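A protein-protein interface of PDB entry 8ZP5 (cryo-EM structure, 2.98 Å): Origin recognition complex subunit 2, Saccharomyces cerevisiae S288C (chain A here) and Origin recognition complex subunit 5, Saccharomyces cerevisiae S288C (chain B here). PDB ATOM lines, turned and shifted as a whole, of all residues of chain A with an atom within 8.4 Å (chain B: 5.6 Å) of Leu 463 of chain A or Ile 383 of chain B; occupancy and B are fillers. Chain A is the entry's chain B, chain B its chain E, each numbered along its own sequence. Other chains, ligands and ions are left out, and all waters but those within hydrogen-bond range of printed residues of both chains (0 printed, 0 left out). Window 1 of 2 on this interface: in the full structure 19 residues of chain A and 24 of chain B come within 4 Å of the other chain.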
ATOM      1  N   TYR A 246     -26.950  -9.873 -10.663  1.00  0.00           N
ATOM      2  CA  TYR A 246     -26.839 -11.152 -11.357  1.00  0.00           C
ATOM      3  C   TYR A 246     -27.505 -11.093 -12.724  1.00  0.00           C
ATOM      4  O   TYR A 246     -26.962 -11.603 -13.710  1.00  0.00           O
ATOM      5  CB  TYR A 246     -27.460 -12.262 -10.512  1.00  0.00           C
ATOM      6  CG  TYR A 246     -27.754 -13.532 -11.280  1.00  0.00           C
ATOM      7  CD1 TYR A 246     -26.732 -14.382 -11.672  1.00  0.00           C
ATOM      8  CD2 TYR A 246     -29.054 -13.877 -11.614  1.00  0.00           C
ATOM      9  CE1 TYR A 246     -26.998 -15.543 -12.372  1.00  0.00           C
ATOM     10  CE2 TYR A 246     -29.330 -15.035 -12.315  1.00  0.00           C
ATOM     11  CZ  TYR A 246     -28.298 -15.864 -12.692  1.00  0.00           C
ATOM     12  OH  TYR A 246     -28.566 -17.018 -13.389  1.00  0.00           O
ATOM     13  N   ARG A 433     -18.796 -35.585   1.243  1.00  0.00           N
ATOM     14  CA  ARG A 433     -20.046 -34.867   1.048  1.00  0.00           C
ATOM     15  C   ARG A 433     -21.197 -35.764   0.617  1.00  0.00           C
ATOM     16  O   ARG A 433     -22.339 -35.294   0.569  1.00  0.00           O
ATOM     17  CB  ARG A 433     -19.864 -33.770  -0.006  1.00  0.00           C
ATOM     18  CG  ARG A 433     -19.793 -34.312  -1.425  1.00  0.00           C
ATOM     19  CD  ARG A 433     -19.671 -33.209  -2.458  1.00  0.00           C
ATOM     20  NE  ARG A 433     -18.413 -32.483  -2.339  1.00  0.00           N
ATOM     21  CZ  ARG A 433     -18.037 -31.503  -3.148  1.00  0.00           C
ATOM     22  NH1 ARG A 433     -18.788 -31.121  -4.166  1.00  0.00           N
ATOM     23  NH2 ARG A 433     -16.873 -30.896  -2.934  1.00  0.00           N
ATOM     24  N   ASN A 435     -24.209 -38.579   0.326  1.00  0.00           N
ATOM     25  CA  ASN A 435     -25.348 -38.744   1.223  1.00  0.00           C
ATOM     26  C   ASN A 435     -25.150 -39.893   2.203  1.00  0.00           C
ATOM     27  O   ASN A 435     -25.675 -39.845   3.320  1.00  0.00           O
ATOM     28  CB  ASN A 435     -26.624 -38.961   0.412  1.00  0.00           C
ATOM     29  CG  ASN A 435     -27.871 -38.578   1.178  1.00  0.00           C
ATOM     30  OD1 ASN A 435     -28.278 -39.271   2.110  1.00  0.00           O
ATOM     31  ND2 ASN A 435     -28.486 -37.469   0.789  1.00  0.00           N
ATOM     32  N   GLN A 438     -22.774 -38.675   4.982  1.00  0.00           N
ATOM     33  CA  GLN A 438     -23.515 -37.640   5.695  1.00  0.00           C
ATOM     34  C   GLN A 438     -24.590 -38.247   6.586  1.00  0.00           C
ATOM     35  O   GLN A 438     -24.813 -37.771   7.701  1.00  0.00           O
ATOM     36  CB  GLN A 438     -24.133 -36.648   4.713  1.00  0.00           C
ATOM     37  CG  GLN A 438     -23.115 -35.836   3.940  1.00  0.00           C
ATOM     38  CD  GLN A 438     -22.379 -34.848   4.815  1.00  0.00           C
ATOM     39  OE1 GLN A 438     -22.973 -34.199   5.673  1.00  0.00           O
ATOM     40  NE2 GLN A 438     -21.074 -34.735   4.607  1.00  0.00           N
ATOM     41  N   HIS A 458     -16.810 -25.251   1.321  1.00  0.00           N
ATOM     42  CA  HIS A 458     -17.683 -24.912   0.207  1.00  0.00           C
ATOM     43  C   HIS A 458     -18.705 -23.863   0.627  1.00  0.00           C
ATOM     44  O   HIS A 458     -19.161 -23.829   1.772  1.00  0.00           O
ATOM     45  CB  HIS A 458     -18.397 -26.159  -0.312  1.00  0.00           C
ATOM     46  CG  HIS A 458     -18.823 -26.059  -1.743  1.00  0.00           C
ATOM     47  ND1 HIS A 458     -20.044 -25.543  -2.122  1.00  0.00           N
ATOM     48  CD2 HIS A 458     -18.192 -26.411  -2.888  1.00  0.00           C
ATOM     49  CE1 HIS A 458     -20.145 -25.579  -3.439  1.00  0.00           C
ATOM     50  NE2 HIS A 458     -19.035 -26.103  -3.927  1.00  0.00           N
ATOM     51  N   ILE A 459     -19.064 -22.997  -0.321  1.00  0.00           N
ATOM     52  CA  ILE A 459     -19.977 -21.901  -0.019  1.00  0.00           C
ATOM     53  C   ILE A 459     -21.432 -22.353  -0.046  1.00  0.00           C
ATOM     54  O   ILE A 459     -22.288 -21.706   0.570  1.00  0.00           O
ATOM     55  CB  ILE A 459     -19.737 -20.738  -0.996  1.00  0.00           C
ATOM     56  CG1 ILE A 459     -20.444 -19.472  -0.519  1.00  0.00           C
ATOM     57  CG2 ILE A 459     -20.224 -21.100  -2.385  1.00  0.00           C
ATOM     58  CD1 ILE A 459     -19.996 -18.224  -1.234  1.00  0.00           C
ATOM     59  N   TYR A 460     -21.735 -23.460  -0.725  1.00  0.00           N
ATOM     60  CA  TYR A 460     -23.076 -24.025  -0.765  1.00  0.00           C
ATOM     61  C   TYR A 460     -23.232 -25.208   0.182  1.00  0.00           C
ATOM     62  O   TYR A 460     -24.148 -26.016   0.006  1.00  0.00           O
ATOM     63  CB  TYR A 460     -23.434 -24.448  -2.190  1.00  0.00           C
ATOM     64  CG  TYR A 460     -23.773 -23.298  -3.109  1.00  0.00           C
ATOM     65  CD1 TYR A 460     -24.571 -22.251  -2.674  1.00  0.00           C
ATOM     66  CD2 TYR A 460     -23.296 -23.260  -4.410  1.00  0.00           C
ATOM     67  CE1 TYR A 460     -24.883 -21.199  -3.509  1.00  0.00           C
ATOM     68  CE2 TYR A 460     -23.603 -22.210  -5.251  1.00  0.00           C
ATOM     69  CZ  TYR A 460     -24.397 -21.183  -4.794  1.00  0.00           C
ATOM     70  OH  TYR A 460     -24.707 -20.135  -5.627  1.00  0.00           O
ATOM     71  N   ALA A 461     -22.359 -25.320   1.182  1.00  0.00           N
ATOM     72  CA  ALA A 461     -22.404 -26.445   2.112  1.00  0.00           C
ATOM     73  C   ALA A 461     -23.761 -26.663   2.775  1.00  0.00           C
ATOM     74  O   ALA A 461     -24.184 -27.828   2.867  1.00  0.00           O
ATOM     75  CB  ALA A 461     -21.312 -26.274   3.177  1.00  0.00           C
ATOM     76  N   PRO A 462     -24.487 -25.641   3.246  1.00  0.00           N
ATOM     77  CA  PRO A 462     -25.771 -25.912   3.914  1.00  0.00           C
ATOM     78  C   PRO A 462     -26.786 -26.617   3.033  1.00  0.00           C
ATOM     79  O   PRO A 462     -27.758 -27.172   3.559  1.00  0.00           O
ATOM     80  CB  PRO A 462     -26.263 -24.516   4.318  1.00  0.00           C
ATOM     81  CG  PRO A 462     -25.049 -23.686   4.355  1.00  0.00           C
ATOM     82  CD  PRO A 462     -24.155 -24.206   3.293  1.00  0.00           C
ATOM     83  N   LEU A 463     -26.597 -26.612   1.712  1.00  0.00           N
ATOM     84  CA  LEU A 463     -27.492 -27.344   0.826  1.00  0.00           C
ATOM     85  C   LEU A 463     -27.454 -28.845   1.085  1.00  0.00           C
ATOM     86  O   LEU A 463     -28.389 -29.552   0.698  1.00  0.00           O
ATOM     87  CB  LEU A 463     -27.129 -27.053  -0.632  1.00  0.00           C
ATOM     88  CG  LEU A 463     -28.073 -27.533  -1.733  1.00  0.00           C
ATOM     89  CD1 LEU A 463     -29.516 -27.244  -1.369  1.00  0.00           C
ATOM     90  CD2 LEU A 463     -27.713 -26.886  -3.059  1.00  0.00           C
ATOM     91  N   LEU A 464     -26.402 -29.342   1.738  1.00  0.00           N
ATOM     92  CA  LEU A 464     -26.269 -30.780   1.940  1.00  0.00           C
ATOM     93  C   LEU A 464     -27.340 -31.324   2.879  1.00  0.00           C
ATOM     94  O   LEU A 464     -27.841 -32.435   2.675  1.00  0.00           O
ATOM     95  CB  LEU A 464     -24.881 -31.110   2.486  1.00  0.00           C
ATOM     96  CG  LEU A 464     -23.678 -30.883   1.572  1.00  0.00           C
ATOM     97  CD1 LEU A 464     -22.412 -30.740   2.397  1.00  0.00           C
ATOM     98  CD2 LEU A 464     -23.545 -32.019   0.575  1.00  0.00           C
ATOM     99  N   TRP A 465     -27.703 -30.565   3.909  1.00  0.00           N
ATOM    100  CA  TRP A 465     -28.449 -31.105   5.038  1.00  0.00           C
ATOM    101  C   TRP A 465     -29.890 -30.610   5.007  1.00  0.00           C
ATOM    102  O   TRP A 465     -30.135 -29.400   4.970  1.00  0.00           O
ATOM    103  CB  TRP A 465     -27.782 -30.716   6.354  1.00  0.00           C
ATOM    104  CG  TRP A 465     -26.297 -30.835   6.304  1.00  0.00           C
ATOM    105  CD1 TRP A 465     -25.572 -31.969   6.114  1.00  0.00           C
ATOM    106  CD2 TRP A 465     -25.349 -29.779   6.494  1.00  0.00           C
ATOM    107  NE1 TRP A 465     -24.229 -31.684   6.143  1.00  0.00           N
ATOM    108  CE2 TRP A 465     -24.067 -30.345   6.380  1.00  0.00           C
ATOM    109  CE3 TRP A 465     -25.461 -28.408   6.738  1.00  0.00           C
ATOM    110  CZ2 TRP A 465     -22.905 -29.589   6.502  1.00  0.00           C
ATOM    111  CZ3 TRP A 465     -24.308 -27.660   6.858  1.00  0.00           C
ATOM    112  CH2 TRP A 465     -23.046 -28.251   6.740  1.00  0.00           C
ATOM    113  N   ASP A 466     -30.834 -31.547   5.028  1.00  0.00           N
ATOM    114  CA  ASP A 466     -32.252 -31.229   5.142  1.00  0.00           C
ATOM    115  C   ASP A 466     -32.605 -31.011   6.614  1.00  0.00           C
ATOM    116  O   ASP A 466     -31.729 -30.873   7.471  1.00  0.00           O
ATOM    117  CB  ASP A 466     -33.089 -32.325   4.489  1.00  0.00           C
ATOM    118  CG  ASP A 466     -32.837 -33.696   5.091  1.00  0.00           C
ATOM    119  OD1 ASP A 466     -31.965 -33.816   5.974  1.00  0.00           O
ATOM    120  OD2 ASP A 466     -33.514 -34.659   4.676  1.00  0.00           O
ATOM    121  N   LYS A 469     -31.256 -34.020   8.922  1.00  0.00           N
ATOM    122  CA  LYS A 469     -29.815 -34.041   9.150  1.00  0.00           C
ATOM    123  C   LYS A 469     -29.357 -32.807   9.918  1.00  0.00           C
ATOM    124  O   LYS A 469     -28.464 -32.896  10.767  1.00  0.00           O
ATOM    125  CB  LYS A 469     -29.075 -34.166   7.820  1.00  0.00           C
ATOM    126  CG  LYS A 469     -28.996 -35.596   7.310  1.00  0.00           C
ATOM    127  CD  LYS A 469     -27.900 -35.772   6.277  1.00  0.00           C
ATOM    128  CE  LYS A 469     -28.229 -35.043   4.991  1.00  0.00           C
ATOM    129  NZ  LYS A 469     -27.213 -35.300   3.935  1.00  0.00           N
ATOM    130  N   PHE B 381     -31.916 -25.974 -14.577  1.00  0.00           N
ATOM    131  CA  PHE B 381     -31.314 -24.694 -14.229  1.00  0.00           C
ATOM    132  C   PHE B 381     -30.258 -24.926 -13.154  1.00  0.00           C
ATOM    133  O   PHE B 381     -29.918 -26.066 -12.827  1.00  0.00           O
ATOM    134  CB  PHE B 381     -32.396 -23.706 -13.779  1.00  0.00           C
ATOM    135  CG  PHE B 381     -33.275 -24.229 -12.681  1.00  0.00           C
ATOM    136  CD1 PHE B 381     -32.899 -24.101 -11.357  1.00  0.00           C
ATOM    137  CD2 PHE B 381     -34.477 -24.846 -12.972  1.00  0.00           C
ATOM    138  CE1 PHE B 381     -33.701 -24.583 -10.349  1.00  0.00           C
ATOM    139  CE2 PHE B 381     -35.286 -25.328 -11.964  1.00  0.00           C
ATOM    140  CZ  PHE B 381     -34.895 -25.195 -10.650  1.00  0.00           C
ATOM    141  N   ALA B 382     -29.745 -23.834 -12.596  1.00  0.00           N
ATOM    142  CA  ALA B 382     -28.690 -23.874 -11.596  1.00  0.00           C
ATOM    143  C   ALA B 382     -29.193 -23.304 -10.276  1.00  0.00           C
ATOM    144  O   ALA B 382     -30.285 -22.738 -10.187  1.00  0.00           O
ATOM    145  CB  ALA B 382     -27.452 -23.101 -12.070  1.00  0.00           C
ATOM    146  N   ILE B 383     -28.369 -23.465  -9.238  1.00  0.00           N
ATOM    147  CA  ILE B 383     -28.749 -23.013  -7.902  1.00  0.00           C
ATOM    148  C   ILE B 383     -28.766 -21.492  -7.829  1.00  0.00           C
ATOM    149  O   ILE B 383     -29.663 -20.897  -7.217  1.00  0.00           O
ATOM    150  CB  ILE B 383     -27.803 -23.623  -6.851  1.00  0.00           C
ATOM    151  CG1 ILE B 383     -28.214 -25.060  -6.544  1.00  0.00           C
ATOM    152  CG2 ILE B 383     -27.804 -22.798  -5.576  1.00  0.00           C
ATOM    153  CD1 ILE B 383     -29.579 -25.173  -5.912  1.00  0.00           C
ATOM    154  N   GLU B 384     -27.779 -20.837  -8.446  1.00  0.00           N
ATOM    155  CA  GLU B 384     -27.679 -19.384  -8.346  1.00  0.00           C
ATOM    156  C   GLU B 384     -28.882 -18.695  -8.980  1.00  0.00           C
ATOM    157  O   GLU B 384     -29.380 -17.694  -8.452  1.00  0.00           O
ATOM    158  CB  GLU B 384     -26.373 -18.903  -8.981  1.00  0.00           C
ATOM    159  CG  GLU B 384     -26.202 -19.265 -10.447  1.00  0.00           C
ATOM    160  CD  GLU B 384     -25.389 -20.531 -10.642  1.00  0.00           C
ATOM    161  OE1 GLU B 384     -25.152 -21.246  -9.647  1.00  0.00           O
ATOM    162  OE2 GLU B 384     -24.987 -20.809 -11.791  1.00  0.00           O
ATOM    163  N   ARG B 385     -29.368 -19.216 -10.109  1.00  0.00           N
ATOM    164  CA  ARG B 385     -30.553 -18.637 -10.733  1.00  0.00           C
ATOM    165  C   ARG B 385     -31.779 -18.800  -9.844  1.00  0.00           C
ATOM    166  O   ARG B 385     -32.592 -17.873  -9.721  1.00  0.00           O
ATOM    167  CB  ARG B 385     -30.789 -19.272 -12.102  1.00  0.00           C
ATOM    168  CG  ARG B 385     -31.921 -18.638 -12.886  1.00  0.00           C
ATOM    169  CD  ARG B 385     -31.733 -18.823 -14.381  1.00  0.00           C
ATOM    170  NE  ARG B 385     -32.979 -18.631 -15.114  1.00  0.00           N
ATOM    171  CZ  ARG B 385     -33.661 -19.607 -15.698  1.00  0.00           C
ATOM    172  NH1 ARG B 385     -33.242 -20.861 -15.660  1.00  0.00           N
ATOM    173  NH2 ARG B 385     -34.792 -19.318 -16.334  1.00  0.00           N
ATOM    174  N   LEU B 386     -31.930 -19.969  -9.217  1.00  0.00           N
ATOM    175  CA  LEU B 386     -33.041 -20.175  -8.294  1.00  0.00           C
ATOM    176  C   LEU B 386     -32.968 -19.204  -7.125  1.00  0.00           C
ATOM    177  O   LEU B 386     -33.985 -18.630  -6.724  1.00  0.00           O
ATOM    178  CB  LEU B 386     -33.051 -21.620  -7.791  1.00  0.00           C
ATOM    179  CG  LEU B 386     -34.268 -22.085  -6.982  1.00  0.00           C
ATOM    180  CD1 LEU B 386     -34.520 -23.563  -7.193  1.00  0.00           C
ATOM    181  CD2 LEU B 386     -34.083 -21.813  -5.502  1.00  0.00           C
ATOM    182  N   LEU B 387     -31.775 -19.011  -6.562  1.00  0.00           N
ATOM    183  CA  LEU B 387     -31.631 -18.088  -5.440  1.00  0.00           C
ATOM    184  C   LEU B 387     -31.928 -16.656  -5.862  1.00  0.00           C
ATOM    185  O   LEU B 387     -32.561 -15.902  -5.115  1.00  0.00           O
ATOM    186  CB  LEU B 387     -30.227 -18.196  -4.847  1.00  0.00           C
ATOM    187  CG  LEU B 387     -29.859 -19.543  -4.224  1.00  0.00           C
ATOM    188  CD1 LEU B 387     -28.396 -19.555  -3.814  1.00  0.00           C
ATOM    189  CD2 LEU B 387     -30.758 -19.853  -3.037  1.00  0.00           C
ATOM    190  N   ALA B 388     -31.478 -16.261  -7.056  1.00  0.00           N
ATOM    191  CA  ALA B 388     -31.751 -14.912  -7.538  1.00  0.00           C
ATOM    192  C   ALA B 388     -33.243 -14.690  -7.745  1.00  0.00           C
ATOM    193  O   ALA B 388     -33.779 -13.642  -7.368  1.00  0.00           O
ATOM    194  CB  ALA B 388     -30.986 -14.653  -8.832  1.00  0.00           C
ATOM    195  N   PHE B 421     -31.340 -22.674   2.636  1.00  0.00           N
ATOM    196  CA  PHE B 421     -30.717 -23.866   2.072  1.00  0.00           C
ATOM    197  C   PHE B 421     -31.283 -25.134   2.695  1.00  0.00           C
ATOM    198  O   PHE B 421     -31.442 -26.150   2.011  1.00  0.00           O
ATOM    199  CB  PHE B 421     -29.205 -23.801   2.256  1.00  0.00           C
ATOM    200  CG  PHE B 421     -28.511 -22.961   1.230  1.00  0.00           C
ATOM    201  CD1 PHE B 421     -28.205 -23.481  -0.013  1.00  0.00           C
ATOM    202  CD2 PHE B 421     -28.176 -21.649   1.504  1.00  0.00           C
ATOM    203  CE1 PHE B 421     -27.571 -22.712  -0.959  1.00  0.00           C
ATOM    204  CE2 PHE B 421     -27.542 -20.874   0.559  1.00  0.00           C
ATOM    205  CZ  PHE B 421     -27.240 -21.406  -0.673  1.00  0.00           C
ATOM    206  N   LEU B 424     -34.526 -25.703   0.969  1.00  0.00           N
ATOM    207  CA  LEU B 424     -34.300 -26.212  -0.382  1.00  0.00           C
ATOM    208  C   LEU B 424     -33.914 -27.688  -0.365  1.00  0.00           C
ATOM    209  O   LEU B 424     -34.402 -28.481  -1.183  1.00  0.00           O
ATOM    210  CB  LEU B 424     -33.222 -25.377  -1.073  1.00  0.00           C
ATOM    211  CG  LEU B 424     -32.838 -25.758  -2.502  1.00  0.00           C
ATOM    212  CD1 LEU B 424     -34.051 -25.713  -3.413  1.00  0.00           C
ATOM    213  CD2 LEU B 424     -31.756 -24.826  -3.010  1.00  0.00           C
ATOM    214  N   SER B 425     -33.040 -28.078   0.565  1.00  0.00           N
ATOM    215  CA  SER B 425     -32.650 -29.478   0.669  1.00  0.00           C
ATOM    216  C   SER B 425     -33.827 -30.347   1.095  1.00  0.00           C
ATOM    217  O   SER B 425     -33.962 -31.485   0.632  1.00  0.00           O
ATOM    218  CB  SER B 425     -31.489 -29.628   1.649  1.00  0.00           C
ATOM    219  OG  SER B 425     -30.822 -30.861   1.452  1.00  0.00           O
ATOM    220  N   TYR B 443     -24.760 -32.542  -3.985  1.00  0.00           N
ATOM    221  CA  TYR B 443     -25.453 -31.283  -4.234  1.00  0.00           C
ATOM    222  C   TYR B 443     -24.498 -30.154  -4.594  1.00  0.00           C
ATOM    223  O   TYR B 443     -24.918 -29.184  -5.235  1.00  0.00           O
ATOM    224  CB  TYR B 443     -26.269 -30.877  -3.006  1.00  0.00           C
ATOM    225  CG  TYR B 443     -27.329 -31.871  -2.595  1.00  0.00           C
ATOM    226  CD1 TYR B 443     -27.839 -32.792  -3.497  1.00  0.00           C
ATOM    227  CD2 TYR B 443     -27.820 -31.887  -1.298  1.00  0.00           C
ATOM    228  CE1 TYR B 443     -28.806 -33.699  -3.118  1.00  0.00           C
ATOM    229  CE2 TYR B 443     -28.787 -32.788  -0.911  1.00  0.00           C
ATOM    230  CZ  TYR B 443     -29.277 -33.691  -1.823  1.00  0.00           C
ATOM    231  OH  TYR B 443     -30.242 -34.592  -1.435  1.00  0.00           O
ATOM    232  N   LEU B 444     -23.233 -30.255  -4.200  1.00  0.00           N
ATOM    233  CA  LEU B 444     -22.280 -29.168  -4.363  1.00  0.00           C
ATOM    234  C   LEU B 444     -21.529 -29.223  -5.687  1.00  0.00           C
ATOM    235  O   LEU B 444     -20.729 -28.325  -5.964  1.00  0.00           O
ATOM    236  CB  LEU B 444     -21.277 -29.172  -3.205  1.00  0.00           C
ATOM    237  CG  LEU B 444     -21.825 -29.360  -1.788  1.00  0.00           C
ATOM    238  CD1 LEU B 444     -20.760 -29.009  -0.770  1.00  0.00           C
ATOM    239  CD2 LEU B 444     -23.068 -28.524  -1.557  1.00  0.00           C
ATOM    240  N   TRP B 450     -31.014 -28.627 -11.431  1.00  0.00           N
ATOM    241  CA  TRP B 450     -32.254 -28.901 -10.724  1.00  0.00           C
ATOM    242  C   TRP B 450     -33.458 -28.703 -11.639  1.00  0.00           C
ATOM    243  O   TRP B 450     -33.386 -28.021 -12.664  1.00  0.00           O
ATOM    244  CB  TRP B 450     -32.380 -28.005  -9.485  1.00  0.00           C
ATOM    245  CG  TRP B 450     -31.221 -28.132  -8.532  1.00  0.00           C
ATOM    246  CD1 TRP B 450     -29.933 -27.740  -8.750  1.00  0.00           C
ATOM    247  CD2 TRP B 450     -31.250 -28.690  -7.211  1.00  0.00           C
ATOM    248  NE1 TRP B 450     -29.158 -28.021  -7.653  1.00  0.00           N
ATOM    249  CE2 TRP B 450     -29.942 -28.604  -6.695  1.00  0.00           C
ATOM    250  CE3 TRP B 450     -32.251 -29.254  -6.418  1.00  0.00           C
ATOM    251  CZ2 TRP B 450     -29.613 -29.059  -5.421  1.00  0.00           C
ATOM    252  CZ3 TRP B 450     -31.922 -29.706  -5.154  1.00  0.00           C
ATOM    253  CH2 TRP B 450     -30.615 -29.606  -4.668  1.00  0.00           C
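Among the printed residues, merely in contact across the chains: Tyr 246 of chain A with Arg 385 of chain B, Tyr 246 of chain A with Ala 388 of chain B, Arg 433 of chain A with Leu 444 of chain B, Tyr 460 of chain A with Ile 383 of chain B, Tyr 460 of chain A with Glu 384 of chain B, Tyr 460 of chain A with Leu 387 of chain B, Tyr 460 of chain A with Phe 421 of chain B, Tyr 460 of chain A with Leu 444 of chain B, Pro 462 of chain A with Phe 421 of chain B, Leu 463 of chain A with Ile 383 of chain B, Leu 463 of chain A with Phe 421 of chain B, Leu 463 of chain A with Leu 424 of chain B, Leu 463 of chain A with Tyr 443 of chain B, Leu 463 of chain A with Trp 450 of chain B, Leu 464 of chain A with Ser 425 of chain B, Leu 464 of chain A with Tyr 443 of chain B, Leu 464 of chain A with Leu 444 of chain B, Trp 465 of chain A with Ser 425 of chain B and Asp 466 of chain A with Ser 425 of chain B.
The backbone carbonyl oxygen of Leu 444 of chain B is in hydrogen-bond range of a ring nitrogen (NE2) of His 458 of chain A (3.5 Å).
The backbone carbonyl oxygen (O) of Leu 463 of chain A sits at hydrogen-bond distance from the side-chain hydroxyl (OG) of Ser 425 of chain B (2.9 Å).
Printed residues of chain B within 4 Å of Leu 463 of chain A: Ile 383 (3.8 Å), Phe 421 (3.8 Å), Leu 424 (3.7 Å), Ser 425 (2.9 Å), Tyr 443 (3.1 Å) and Trp 450 (3.7 Å).
Of chain A, only Tyr 460 (3.9 Å) and Leu 463 (3.8 Å) come within 4 Å of Ile 383 of chain B.
Of the printed residues of chain A, Tyr 443 of chain B touches Leu 463 (3.1 Å) and Leu 464 (3.7 Å).
Of the printed residues of chain B, Tyr 460 of chain A touches Ile 383 (3.9 Å), Glu 384 (3.9 Å), Leu 387 (3.9 Å), Phe 421 (3.4 Å) and Leu 444 (3.1 Å).
The nearest residue of chain A that does not touch Ile 383 of chain B is Tyr 246 of chain A (7.1 Å).
The nearest printed residue of chain A that does not touch Ala 388 of chain B is Tyr 460 of chain A (7.9 Å).
Hydrophobic or aromatic side chains of chain B that line the printed part of chain A: Ile 383, Leu 387, Ala 388, Phe 421, Leu 424, Tyr 443, Leu 444 and Trp 450.
Printed residues of chain A that touch a printed residue of chain B: Tyr 246, Arg 433, His 458, Tyr 460, Pro 462, Leu 463, Leu 464, Trp 465 and Asp 466.
Hydrophobic or aromatic side chains of chain A that line the printed part of chain B: Tyr 246, His 458, Tyr 460, Pro 462, Leu 463 and Leu 464.
Among the printed residues, 21 pairs touch across the chains.
Among the printed residues, no Asp or Glu carboxylate lies within 4 Å of a Lys or Arg side-chain nitrogen of the other chain.
OE1 of Gln 438 of chain A lies within hydrogen-bond range of NE1 of Trp 465 of chain A, 2.9 Å away.
A ring nitrogen (ND1) of His 458 of chain A is in hydrogen-bond range of the backbone NH (N) of Tyr 460 of chain A (3.0 Å).
The backbone carbonyl oxygen (O) of Leu 464 of chain A is in hydrogen-bond range of the side-chain amino group (NZ) of Lys 469 of chain A, at 3.2 Å.
The side-chain carboxylate (OD1) of Asp 466 of chain A sits at hydrogen-bond distance from the backbone NH (N) of Lys 469 of chain A (3.0 Å).
The backbone carbonyl oxygen of Phe 381 of chain B is in hydrogen-bond range of the backbone NH of Trp 450 of chain B, 3.1 Å away.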
